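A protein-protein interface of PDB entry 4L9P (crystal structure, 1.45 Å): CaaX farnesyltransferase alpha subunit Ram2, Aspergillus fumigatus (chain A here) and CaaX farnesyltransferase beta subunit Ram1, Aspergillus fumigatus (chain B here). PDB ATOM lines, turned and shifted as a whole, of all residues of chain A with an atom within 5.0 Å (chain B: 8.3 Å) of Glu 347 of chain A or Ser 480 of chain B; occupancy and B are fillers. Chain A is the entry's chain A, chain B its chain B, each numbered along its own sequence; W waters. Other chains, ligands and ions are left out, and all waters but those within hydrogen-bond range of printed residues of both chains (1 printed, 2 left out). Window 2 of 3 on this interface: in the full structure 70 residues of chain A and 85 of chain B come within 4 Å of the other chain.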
ATOM      1  N   LYS A 335       5.407 -37.366  27.962  1.00  0.00           N
ATOM      2  CA  LYS A 335       4.185 -36.796  27.480  1.00  0.00           C
ATOM      3  C   LYS A 335       3.094 -37.844  27.286  1.00  0.00           C
ATOM      4  O   LYS A 335       1.912 -37.529  27.439  1.00  0.00           O
ATOM      5  CB  LYS A 335       4.455 -35.941  26.228  1.00  0.00           C
ATOM      6  CG  LYS A 335       4.441 -36.624  24.987  1.00  0.00           C
ATOM      7  CD  LYS A 335       4.705 -35.634  23.803  1.00  0.00           C
ATOM      8  CE  LYS A 335       4.311 -36.325  22.510  1.00  0.00           C
ATOM      9  NZ  LYS A 335       4.652 -35.520  21.378  1.00  0.00           N
ATOM     10  N   ARG A 343       2.329 -32.311  29.041  1.00  0.00           N
ATOM     11  CA  ARG A 343       2.610 -32.554  27.618  1.00  0.00           C
ATOM     12  C   ARG A 343       3.086 -31.307  26.864  1.00  0.00           C
ATOM     13  O   ARG A 343       4.005 -31.373  26.041  1.00  0.00           O
ATOM     14  CB  ARG A 343       1.324 -33.054  26.998  1.00  0.00           C
ATOM     15  CG  ARG A 343       1.363 -33.183  25.494  1.00  0.00           C
ATOM     16  CD  ARG A 343       0.038 -33.834  25.054  1.00  0.00           C
ATOM     17  NE  ARG A 343      -0.084 -33.954  23.615  1.00  0.00           N
ATOM     18  CZ  ARG A 343      -1.168 -34.414  22.983  1.00  0.00           C
ATOM     19  NH1 ARG A 343      -2.262 -34.782  23.674  1.00  0.00           N
ATOM     20  NH2 ARG A 343      -1.173 -34.466  21.657  1.00  0.00           N
ATOM     21  N   ASN A 344       2.462 -30.139  27.126  1.00  0.00           N
ATOM     22  CA  ASN A 344       2.798 -28.958  26.308  1.00  0.00           C
ATOM     23  C   ASN A 344       4.196 -28.457  26.647  1.00  0.00           C
ATOM     24  O   ASN A 344       4.901 -27.907  25.787  1.00  0.00           O
ATOM     25  CB  ASN A 344       1.765 -27.823  26.421  1.00  0.00           C
ATOM     26  CG  ASN A 344       0.444 -28.207  25.754  1.00  0.00           C
ATOM     27  OD1 ASN A 344       0.446 -28.900  24.699  1.00  0.00           O
ATOM     28  ND2 ASN A 344      -0.672 -27.890  26.384  1.00  0.00           N
ATOM     29  N   TYR A 345       4.616 -28.636  27.911  1.00  0.00           N
ATOM     30  CA  TYR A 345       5.987 -28.289  28.254  1.00  0.00           C
ATOM     31  C   TYR A 345       6.979 -29.321  27.686  1.00  0.00           C
ATOM     32  O   TYR A 345       8.035 -28.952  27.135  1.00  0.00           O
ATOM     33  CB  TYR A 345       6.111 -28.184  29.812  1.00  0.00           C
ATOM     34  CG  TYR A 345       7.572 -28.037  30.223  1.00  0.00           C
ATOM     35  CD1 TYR A 345       8.307 -26.862  29.905  1.00  0.00           C
ATOM     36  CD2 TYR A 345       8.231 -29.077  30.869  1.00  0.00           C
ATOM     37  CE1 TYR A 345       9.651 -26.764  30.214  1.00  0.00           C
ATOM     38  CE2 TYR A 345       9.594 -28.978  31.193  1.00  0.00           C
ATOM     39  CZ  TYR A 345      10.271 -27.829  30.854  1.00  0.00           C
ATOM     40  OH  TYR A 345      11.615 -27.732  31.149  1.00  0.00           O
ATOM     41  N   TRP A 346       6.648 -30.609  27.775  1.00  0.00           N
ATOM     42  CA  TRP A 346       7.544 -31.611  27.146  1.00  0.00           C
ATOM     43  C   TRP A 346       7.638 -31.349  25.627  1.00  0.00           C
ATOM     44  O   TRP A 346       8.740 -31.475  25.068  1.00  0.00           O
ATOM     45  CB  TRP A 346       7.050 -33.032  27.337  1.00  0.00           C
ATOM     46  CG  TRP A 346       6.768 -33.381  28.822  1.00  0.00           C
ATOM     47  CD1 TRP A 346       5.658 -34.008  29.281  1.00  0.00           C
ATOM     48  CD2 TRP A 346       7.624 -33.170  29.991  1.00  0.00           C
ATOM     49  NE1 TRP A 346       5.725 -34.191  30.670  1.00  0.00           N
ATOM     50  CE2 TRP A 346       6.929 -33.709  31.122  1.00  0.00           C
ATOM     51  CE3 TRP A 346       8.896 -32.583  30.198  1.00  0.00           C
ATOM     52  CZ2 TRP A 346       7.454 -33.654  32.421  1.00  0.00           C
ATOM     53  CZ3 TRP A 346       9.416 -32.553  31.492  1.00  0.00           C
ATOM     54  CH2 TRP A 346       8.700 -33.058  32.580  1.00  0.00           C
ATOM     55  N   GLU A 347       6.541 -30.954  24.981  1.00  0.00           N
ATOM     56  CA  GLU A 347       6.597 -30.737  23.531  1.00  0.00           C
ATOM     57  C   GLU A 347       7.406 -29.474  23.231  1.00  0.00           C
ATOM     58  O   GLU A 347       8.097 -29.427  22.219  1.00  0.00           O
ATOM     59  CB  GLU A 347       5.194 -30.703  22.899  1.00  0.00           C
ATOM     60  CG  GLU A 347       4.499 -32.066  22.922  1.00  0.00           C
ATOM     61  CD  GLU A 347       3.096 -32.119  22.285  1.00  0.00           C
ATOM     62  OE1 GLU A 347       2.461 -31.069  22.038  1.00  0.00           O
ATOM     63  OE2 GLU A 347       2.605 -33.240  22.088  1.00  0.00           O
ATOM     64  N   TYR A 348       7.321 -28.473  24.111  1.00  0.00           N
ATOM     65  CA  TYR A 348       8.169 -27.259  23.968  1.00  0.00           C
ATOM     66  C   TYR A 348       9.665 -27.672  24.039  1.00  0.00           C
ATOM     67  O   TYR A 348      10.495 -27.205  23.230  1.00  0.00           O
ATOM     68  CB  TYR A 348       7.826 -26.237  25.055  1.00  0.00           C
ATOM     69  CG  TYR A 348       8.756 -25.069  25.162  1.00  0.00           C
ATOM     70  CD1 TYR A 348       8.674 -24.035  24.247  1.00  0.00           C
ATOM     71  CD2 TYR A 348       9.688 -24.965  26.215  1.00  0.00           C
ATOM     72  CE1 TYR A 348       9.502 -22.916  24.339  1.00  0.00           C
ATOM     73  CE2 TYR A 348      10.532 -23.852  26.311  1.00  0.00           C
ATOM     74  CZ  TYR A 348      10.424 -22.820  25.384  1.00  0.00           C
ATOM     75  OH  TYR A 348      11.255 -21.715  25.459  1.00  0.00           O
ATOM     76  N   ARG A 349      10.015 -28.562  24.977  1.00  0.00           N
ATOM     77  CA  ARG A 349      11.391 -29.050  25.080  1.00  0.00           C
ATOM     78  C   ARG A 349      11.772 -29.808  23.817  1.00  0.00           C
ATOM     79  O   ARG A 349      12.862 -29.610  23.294  1.00  0.00           O
ATOM     80  CB  ARG A 349      11.627 -29.938  26.301  1.00  0.00           C
ATOM     81  CG  ARG A 349      11.525 -29.149  27.628  1.00  0.00           C
ATOM     82  CD  ARG A 349      12.767 -28.248  27.835  1.00  0.00           C
ATOM     83  NE  ARG A 349      13.942 -29.091  28.058  1.00  0.00           N
ATOM     84  CZ  ARG A 349      15.107 -28.975  27.427  1.00  0.00           C
ATOM     85  NH1 ARG A 349      15.289 -28.049  26.464  1.00  0.00           N
ATOM     86  NH2 ARG A 349      16.114 -29.800  27.752  1.00  0.00           N
ATOM     87  N   ILE A 350      10.881 -30.672  23.320  1.00  0.00           N
ATOM     88  CA  ILE A 350      11.150 -31.385  22.039  1.00  0.00           C
ATOM     89  C   ILE A 350      11.397 -30.372  20.915  1.00  0.00           C
ATOM     90  O   ILE A 350      12.328 -30.548  20.122  1.00  0.00           O
ATOM     91  CB  ILE A 350       9.980 -32.311  21.665  1.00  0.00           C
ATOM     92  CG1 ILE A 350       9.915 -33.475  22.679  1.00  0.00           C
ATOM     93  CG2 ILE A 350      10.167 -32.856  20.235  1.00  0.00           C
ATOM     94  CD1 ILE A 350       8.673 -34.351  22.610  1.00  0.00           C
ATOM     95  N   ARG A 351      10.620 -29.303  20.842  1.00  0.00           N
ATOM     96  CA  ARG A 351      10.806 -28.304  19.781  1.00  0.00           C
ATOM     97  C   ARG A 351      12.162 -27.621  19.924  1.00  0.00           C
ATOM     98  O   ARG A 351      12.837 -27.363  18.938  1.00  0.00           O
ATOM     99  CB  ARG A 351       9.684 -27.247  19.789  1.00  0.00           C
ATOM    100  CG  ARG A 351       8.313 -27.827  19.451  1.00  0.00           C
ATOM    101  CD  ARG A 351       7.278 -26.776  18.980  1.00  0.00           C
ATOM    102  NE  ARG A 351       7.034 -25.723  19.956  1.00  0.00           N
ATOM    103  CZ  ARG A 351       6.166 -25.812  20.967  1.00  0.00           C
ATOM    104  NH1 ARG A 351       5.481 -26.922  21.117  1.00  0.00           N
ATOM    105  NH2 ARG A 351       5.985 -24.788  21.828  1.00  0.00           N
ATOM    106  N   VAL B 397       4.881 -19.512  21.558  1.00  0.00           N
ATOM    107  CA  VAL B 397       5.146 -20.804  22.191  1.00  0.00           C
ATOM    108  C   VAL B 397       3.819 -21.465  22.609  1.00  0.00           C
ATOM    109  O   VAL B 397       3.794 -22.676  22.882  1.00  0.00           O
ATOM    110  CB  VAL B 397       6.086 -20.670  23.451  1.00  0.00           C
ATOM    111  CG1 VAL B 397       7.471 -20.139  23.077  1.00  0.00           C
ATOM    112  CG2 VAL B 397       5.440 -19.783  24.574  1.00  0.00           C
ATOM    113  N   ASN B 399       0.391 -22.296  24.894  1.00  0.00           N
ATOM    114  CA  ASN B 399       0.180 -22.568  26.309  1.00  0.00           C
ATOM    115  C   ASN B 399       1.017 -23.732  26.701  1.00  0.00           C
ATOM    116  O   ASN B 399       0.933 -24.787  26.065  1.00  0.00           O
ATOM    117  CB  ASN B 399      -1.286 -22.859  26.549  1.00  0.00           C
ATOM    118  CG  ASN B 399      -2.113 -21.688  26.204  1.00  0.00           C
ATOM    119  OD1 ASN B 399      -1.856 -20.588  26.758  1.00  0.00           O
ATOM    120  ND2 ASN B 399      -3.060 -21.851  25.237  1.00  0.00           N
ATOM    121  N   LEU B 400       1.851 -23.545  27.713  1.00  0.00           N
ATOM    122  CA  LEU B 400       2.803 -24.554  28.132  1.00  0.00           C
ATOM    123  C   LEU B 400       2.324 -25.443  29.293  1.00  0.00           C
ATOM    124  O   LEU B 400       3.112 -26.163  29.851  1.00  0.00           O
ATOM    125  CB  LEU B 400       4.169 -23.886  28.440  1.00  0.00           C
ATOM    126  CG  LEU B 400       4.805 -23.234  27.181  1.00  0.00           C
ATOM    127  CD1 LEU B 400       6.146 -22.588  27.616  1.00  0.00           C
ATOM    128  CD2 LEU B 400       5.022 -24.212  26.041  1.00  0.00           C
ATOM    129  N   TYR B 401       1.045 -25.357  29.635  1.00  0.00           N
ATOM    130  CA  TYR B 401       0.394 -26.132  30.679  1.00  0.00           C
ATOM    131  C   TYR B 401      -0.898 -26.676  30.026  1.00  0.00           C
ATOM    132  O   TYR B 401      -1.202 -26.361  28.865  1.00  0.00           O
ATOM    133  CB  TYR B 401       0.026 -25.265  31.911  1.00  0.00           C
ATOM    134  CG  TYR B 401      -0.988 -24.202  31.593  1.00  0.00           C
ATOM    135  CD1 TYR B 401      -0.654 -23.042  30.935  1.00  0.00           C
ATOM    136  CD2 TYR B 401      -2.304 -24.373  32.010  1.00  0.00           C
ATOM    137  CE1 TYR B 401      -1.608 -22.062  30.626  1.00  0.00           C
ATOM    138  CE2 TYR B 401      -3.280 -23.378  31.744  1.00  0.00           C
ATOM    139  CZ  TYR B 401      -2.932 -22.221  31.059  1.00  0.00           C
ATOM    140  OH  TYR B 401      -3.941 -21.278  30.801  1.00  0.00           O
ATOM    141  N   SER B 402      -1.658 -27.474  30.781  1.00  0.00           N
ATOM    142  CA  SER B 402      -2.898 -28.071  30.281  1.00  0.00           C
ATOM    143  C   SER B 402      -4.101 -27.228  30.663  1.00  0.00           C
ATOM    144  O   SER B 402      -4.587 -27.270  31.812  1.00  0.00           O
ATOM    145  CB  SER B 402      -3.053 -29.512  30.834  1.00  0.00           C
ATOM    146  OG  SER B 402      -4.332 -30.013  30.428  1.00  0.00           O
ATOM    147  N   ARG B 403      -4.659 -26.515  29.681  1.00  0.00           N
ATOM    148  CA  ARG B 403      -5.898 -25.782  29.929  1.00  0.00           C
ATOM    149  C   ARG B 403      -7.061 -26.733  30.218  1.00  0.00           C
ATOM    150  O   ARG B 403      -7.920 -26.438  31.060  1.00  0.00           O
ATOM    151  CB  ARG B 403      -6.234 -24.864  28.730  1.00  0.00           C
ATOM    152  CG  ARG B 403      -5.277 -23.664  28.576  1.00  0.00           C
ATOM    153  CD  ARG B 403      -5.796 -22.682  27.409  1.00  0.00           C
ATOM    154  NE  ARG B 403      -5.916 -23.293  26.127  1.00  0.00           N
ATOM    155  CZ  ARG B 403      -7.012 -23.308  25.391  1.00  0.00           C
ATOM    156  NH1 ARG B 403      -8.158 -22.645  25.748  1.00  0.00           N
ATOM    157  NH2 ARG B 403      -6.948 -23.922  24.225  1.00  0.00           N
ATOM    158  N   GLU B 404      -7.057 -27.888  29.562  1.00  0.00           N
ATOM    159  CA  GLU B 404      -8.102 -28.885  29.806  1.00  0.00           C
ATOM    160  C   GLU B 404      -8.052 -29.294  31.292  1.00  0.00           C
ATOM    161  O   GLU B 404      -9.088 -29.349  31.937  1.00  0.00           O
ATOM    162  CB  GLU B 404      -7.847 -30.138  28.934  1.00  0.00           C
ATOM    163  CG  GLU B 404      -8.787 -31.280  29.309  1.00  0.00           C
ATOM    164  CD  GLU B 404      -8.725 -32.508  28.418  1.00  0.00           C
ATOM    165  OE1 GLU B 404      -7.830 -32.559  27.553  1.00  0.00           O
ATOM    166  OE2 GLU B 404      -9.640 -33.360  28.551  1.00  0.00           O
ATOM    167  N   GLY B 405      -6.859 -29.663  31.775  1.00  0.00           N
ATOM    168  CA  GLY B 405      -6.765 -30.100  33.173  1.00  0.00           C
ATOM    169  C   GLY B 405      -7.257 -29.056  34.164  1.00  0.00           C
ATOM    170  O   GLY B 405      -8.026 -29.339  35.089  1.00  0.00           O
ATOM    171  N   GLY B 477     -13.142 -31.947  19.839  1.00  0.00           N
ATOM    172  CA  GLY B 477     -12.107 -32.934  19.564  1.00  0.00           C
ATOM    173  C   GLY B 477     -11.055 -32.981  20.662  1.00  0.00           C
ATOM    174  O   GLY B 477     -11.025 -32.188  21.612  1.00  0.00           O
ATOM    175  N   GLN B 478     -10.152 -33.921  20.517  1.00  0.00           N
ATOM    176  CA  GLN B 478      -9.116 -34.134  21.491  1.00  0.00           C
ATOM    177  C   GLN B 478      -7.907 -33.327  21.047  1.00  0.00           C
ATOM    178  O   GLN B 478      -7.773 -32.964  19.889  1.00  0.00           O
ATOM    179  CB  GLN B 478      -8.821 -35.637  21.549  1.00  0.00           C
ATOM    180  CG  GLN B 478      -9.478 -36.334  22.787  1.00  0.00           C
ATOM    181  CD  GLN B 478      -9.005 -37.803  22.957  1.00  0.00           C
ATOM    182  OE1 GLN B 478      -8.991 -38.572  21.972  1.00  0.00           O
ATOM    183  NE2 GLN B 478      -8.619 -38.197  24.213  1.00  0.00           N
ATOM    184  N   GLY B 479      -7.008 -33.028  21.960  1.00  0.00           N
ATOM    185  CA  GLY B 479      -5.862 -32.240  21.584  1.00  0.00           C
ATOM    186  C   GLY B 479      -5.105 -31.902  22.833  1.00  0.00           C
ATOM    187  O   GLY B 479      -5.617 -32.025  23.940  1.00  0.00           O
ATOM    188  N   SER B 480      -3.890 -31.443  22.657  1.00  0.00           N
ATOM    189  CA  SER B 480      -3.077 -31.132  23.847  1.00  0.00           C
ATOM    190  C   SER B 480      -3.341 -29.741  24.413  1.00  0.00           C
ATOM    191  O   SER B 480      -2.981 -29.470  25.564  1.00  0.00           O
ATOM    192  CB  SER B 480      -1.609 -31.224  23.544  1.00  0.00           C
ATOM    193  OG  SER B 480      -1.158 -30.151  22.726  1.00  0.00           O
ATOM    194  N   ASP B 481      -3.902 -28.865  23.595  1.00  0.00           N
ATOM    195  CA  ASP B 481      -4.165 -27.489  24.030  1.00  0.00           C
ATOM    196  C   ASP B 481      -5.555 -27.081  23.617  1.00  0.00           C
ATOM    197  O   ASP B 481      -5.754 -26.448  22.575  1.00  0.00           O
ATOM    198  CB  ASP B 481      -3.090 -26.540  23.506  1.00  0.00           C
ATOM    199  CG  ASP B 481      -3.296 -25.118  23.973  1.00  0.00           C
ATOM    200  OD1 ASP B 481      -3.903 -24.885  25.045  1.00  0.00           O
ATOM    201  OD2 ASP B 481      -2.845 -24.207  23.257  1.00  0.00           O
ATOM    202  N   ILE B 482      -6.533 -27.476  24.438  1.00  0.00           N
ATOM    203  CA  ILE B 482      -7.926 -27.298  24.061  1.00  0.00           C
ATOM    204  C   ILE B 482      -8.762 -26.635  25.129  1.00  0.00           C
ATOM    205  O   ILE B 482      -8.419 -26.634  26.365  1.00  0.00           O
ATOM    206  CB  ILE B 482      -8.600 -28.636  23.695  1.00  0.00           C
ATOM    207  CG1 ILE B 482      -8.410 -29.657  24.839  1.00  0.00           C
ATOM    208  CG2 ILE B 482      -8.089 -29.155  22.346  1.00  0.00           C
ATOM    209  CD1 ILE B 482      -9.234 -31.002  24.646  1.00  0.00           C
ATOM    210  N   GLY B 483      -9.828 -26.013  24.663  1.00  0.00           N
ATOM    211  CA  GLY B 483     -10.760 -25.337  25.530  1.00  0.00           C
ATOM    212  C   GLY B 483     -11.947 -26.233  25.767  1.00  0.00           C
ATOM    213  O   GLY B 483     -12.771 -26.449  24.861  1.00  0.00           O
HETATM  214  O   HOH W   1      -1.691 -30.840  27.585  1.00  0.00           O
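The side-chain amide nitrogen (ND2) of Asn 344 of chain A lies within hydrogen-bond range of the backbone carbonyl oxygen (O) of Tyr 401 of chain B (3.0 Å). The side-chain amide oxygen (OD1) of Asn 344 of chain A sits at hydrogen-bond distance from the side-chain hydroxyl (OG) of Ser 480 of chain B (2.8 Å). N of Tyr 345 of chain A sits at hydrogen-bond distance from O of Leu 400 of chain B, at 3.5 Å. O of Val 397 of chain B lies within hydrogen-bond range of NH2 of Arg 351 of chain A (3.2 Å).
OE2 of Glu 347 of chain A lies within salt-bridge range of NZ of Lys 335 of chain A, 3.1 Å away. The guanidinium group (NE) of Arg 343 of chain A lies within salt-bridge range of the side-chain carboxylate (OE2) of Glu 347 of chain A, 3.2 Å away. The side-chain amide nitrogen (ND2) of Asn 399 of chain B lies close to the guanidinium group (NE) of Arg 403 of chain B (3.3 Å). The side-chain carboxylate (OD2) of Asp 481 of chain B is in hydrogen-bond range of the side-chain amide nitrogen (ND2) of Asn 399 of chain B (3.1 Å). The guanidinium group (NE) of Arg 403 of chain B is in salt-bridge range of the side-chain carboxylate (OD1) of Asp 481 of chain B, at 2.8 Å.
Arg 343 of chain A touches Ser 480 of chain B. Asn 399 of chain B touches Asn 344 of chain A. Leu 400 of chain B touches Asn 344 of chain A (CD2 to O, 3.7 Å). Asn 344 of chain A touches Asp 481 of chain B (ND2 to CB, 3.99 Å). Glu 347 of chain A touches Ser 480 of chain B (OE1 to OG, 3.8 Å). Tyr 348 of chain A touches Val 397 of chain B (CE1 to CG1, 3.7 Å). Tyr 348 of chain A touches Leu 400 of chain B.
Of the printed residues of chain B, Glu 347 of chain A touches Ser 480. Of the printed residues of chain A, Ser 480 of chain B touches Arg 343 (3.1 Å), Asn 344 (2.8 Å) and Glu 347 (3.8 Å). Of the printed residues of chain A, Asn 399 of chain B touches Asn 344 (3.2 Å). Printed residues of chain A within 4 Å of Tyr 401 of chain B: Asn 344. Of the printed residues of chain B, Tyr 345 of chain A touches Leu 400 (3.5 Å). Of the printed residues of chain B, Asn 344 of chain A touches Asn 399 (3.2 Å), Leu 400 (3.7 Å), Tyr 401 (3.0 Å), Ser 480 (2.8 Å) and Asp 481 (3.99 Å). The nearest printed residue of chain A that does not touch Ser 480 of chain B is Arg 351 of chain A (7.6 Å). The nearest printed residue of chain A that does not touch Tyr 401 of chain B is Tyr 345 of chain A (5.1 Å).
Hydrophobic or aromatic side chains of chain A that line the printed part of chain B: Tyr 345 and Tyr 348. Of the 15 printed residues of chain B, 6 touch a printed residue of chain A. Hydrophobic or aromatic side chains of chain B that line the printed part of chain A: Val 397 and Leu 400. Among the printed residues, no Asp or Glu carboxylate lies within 4 Å of a Lys or Arg side-chain nitrogen of the other chain.
Water W1 lies within hydrogen-bond range of the backbone carbonyl oxygen (O) of Ser 480 of chain B (2.8 Å) and the side-chain amide nitrogen (ND2) of Asn 344 of chain A (3.3 Å).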
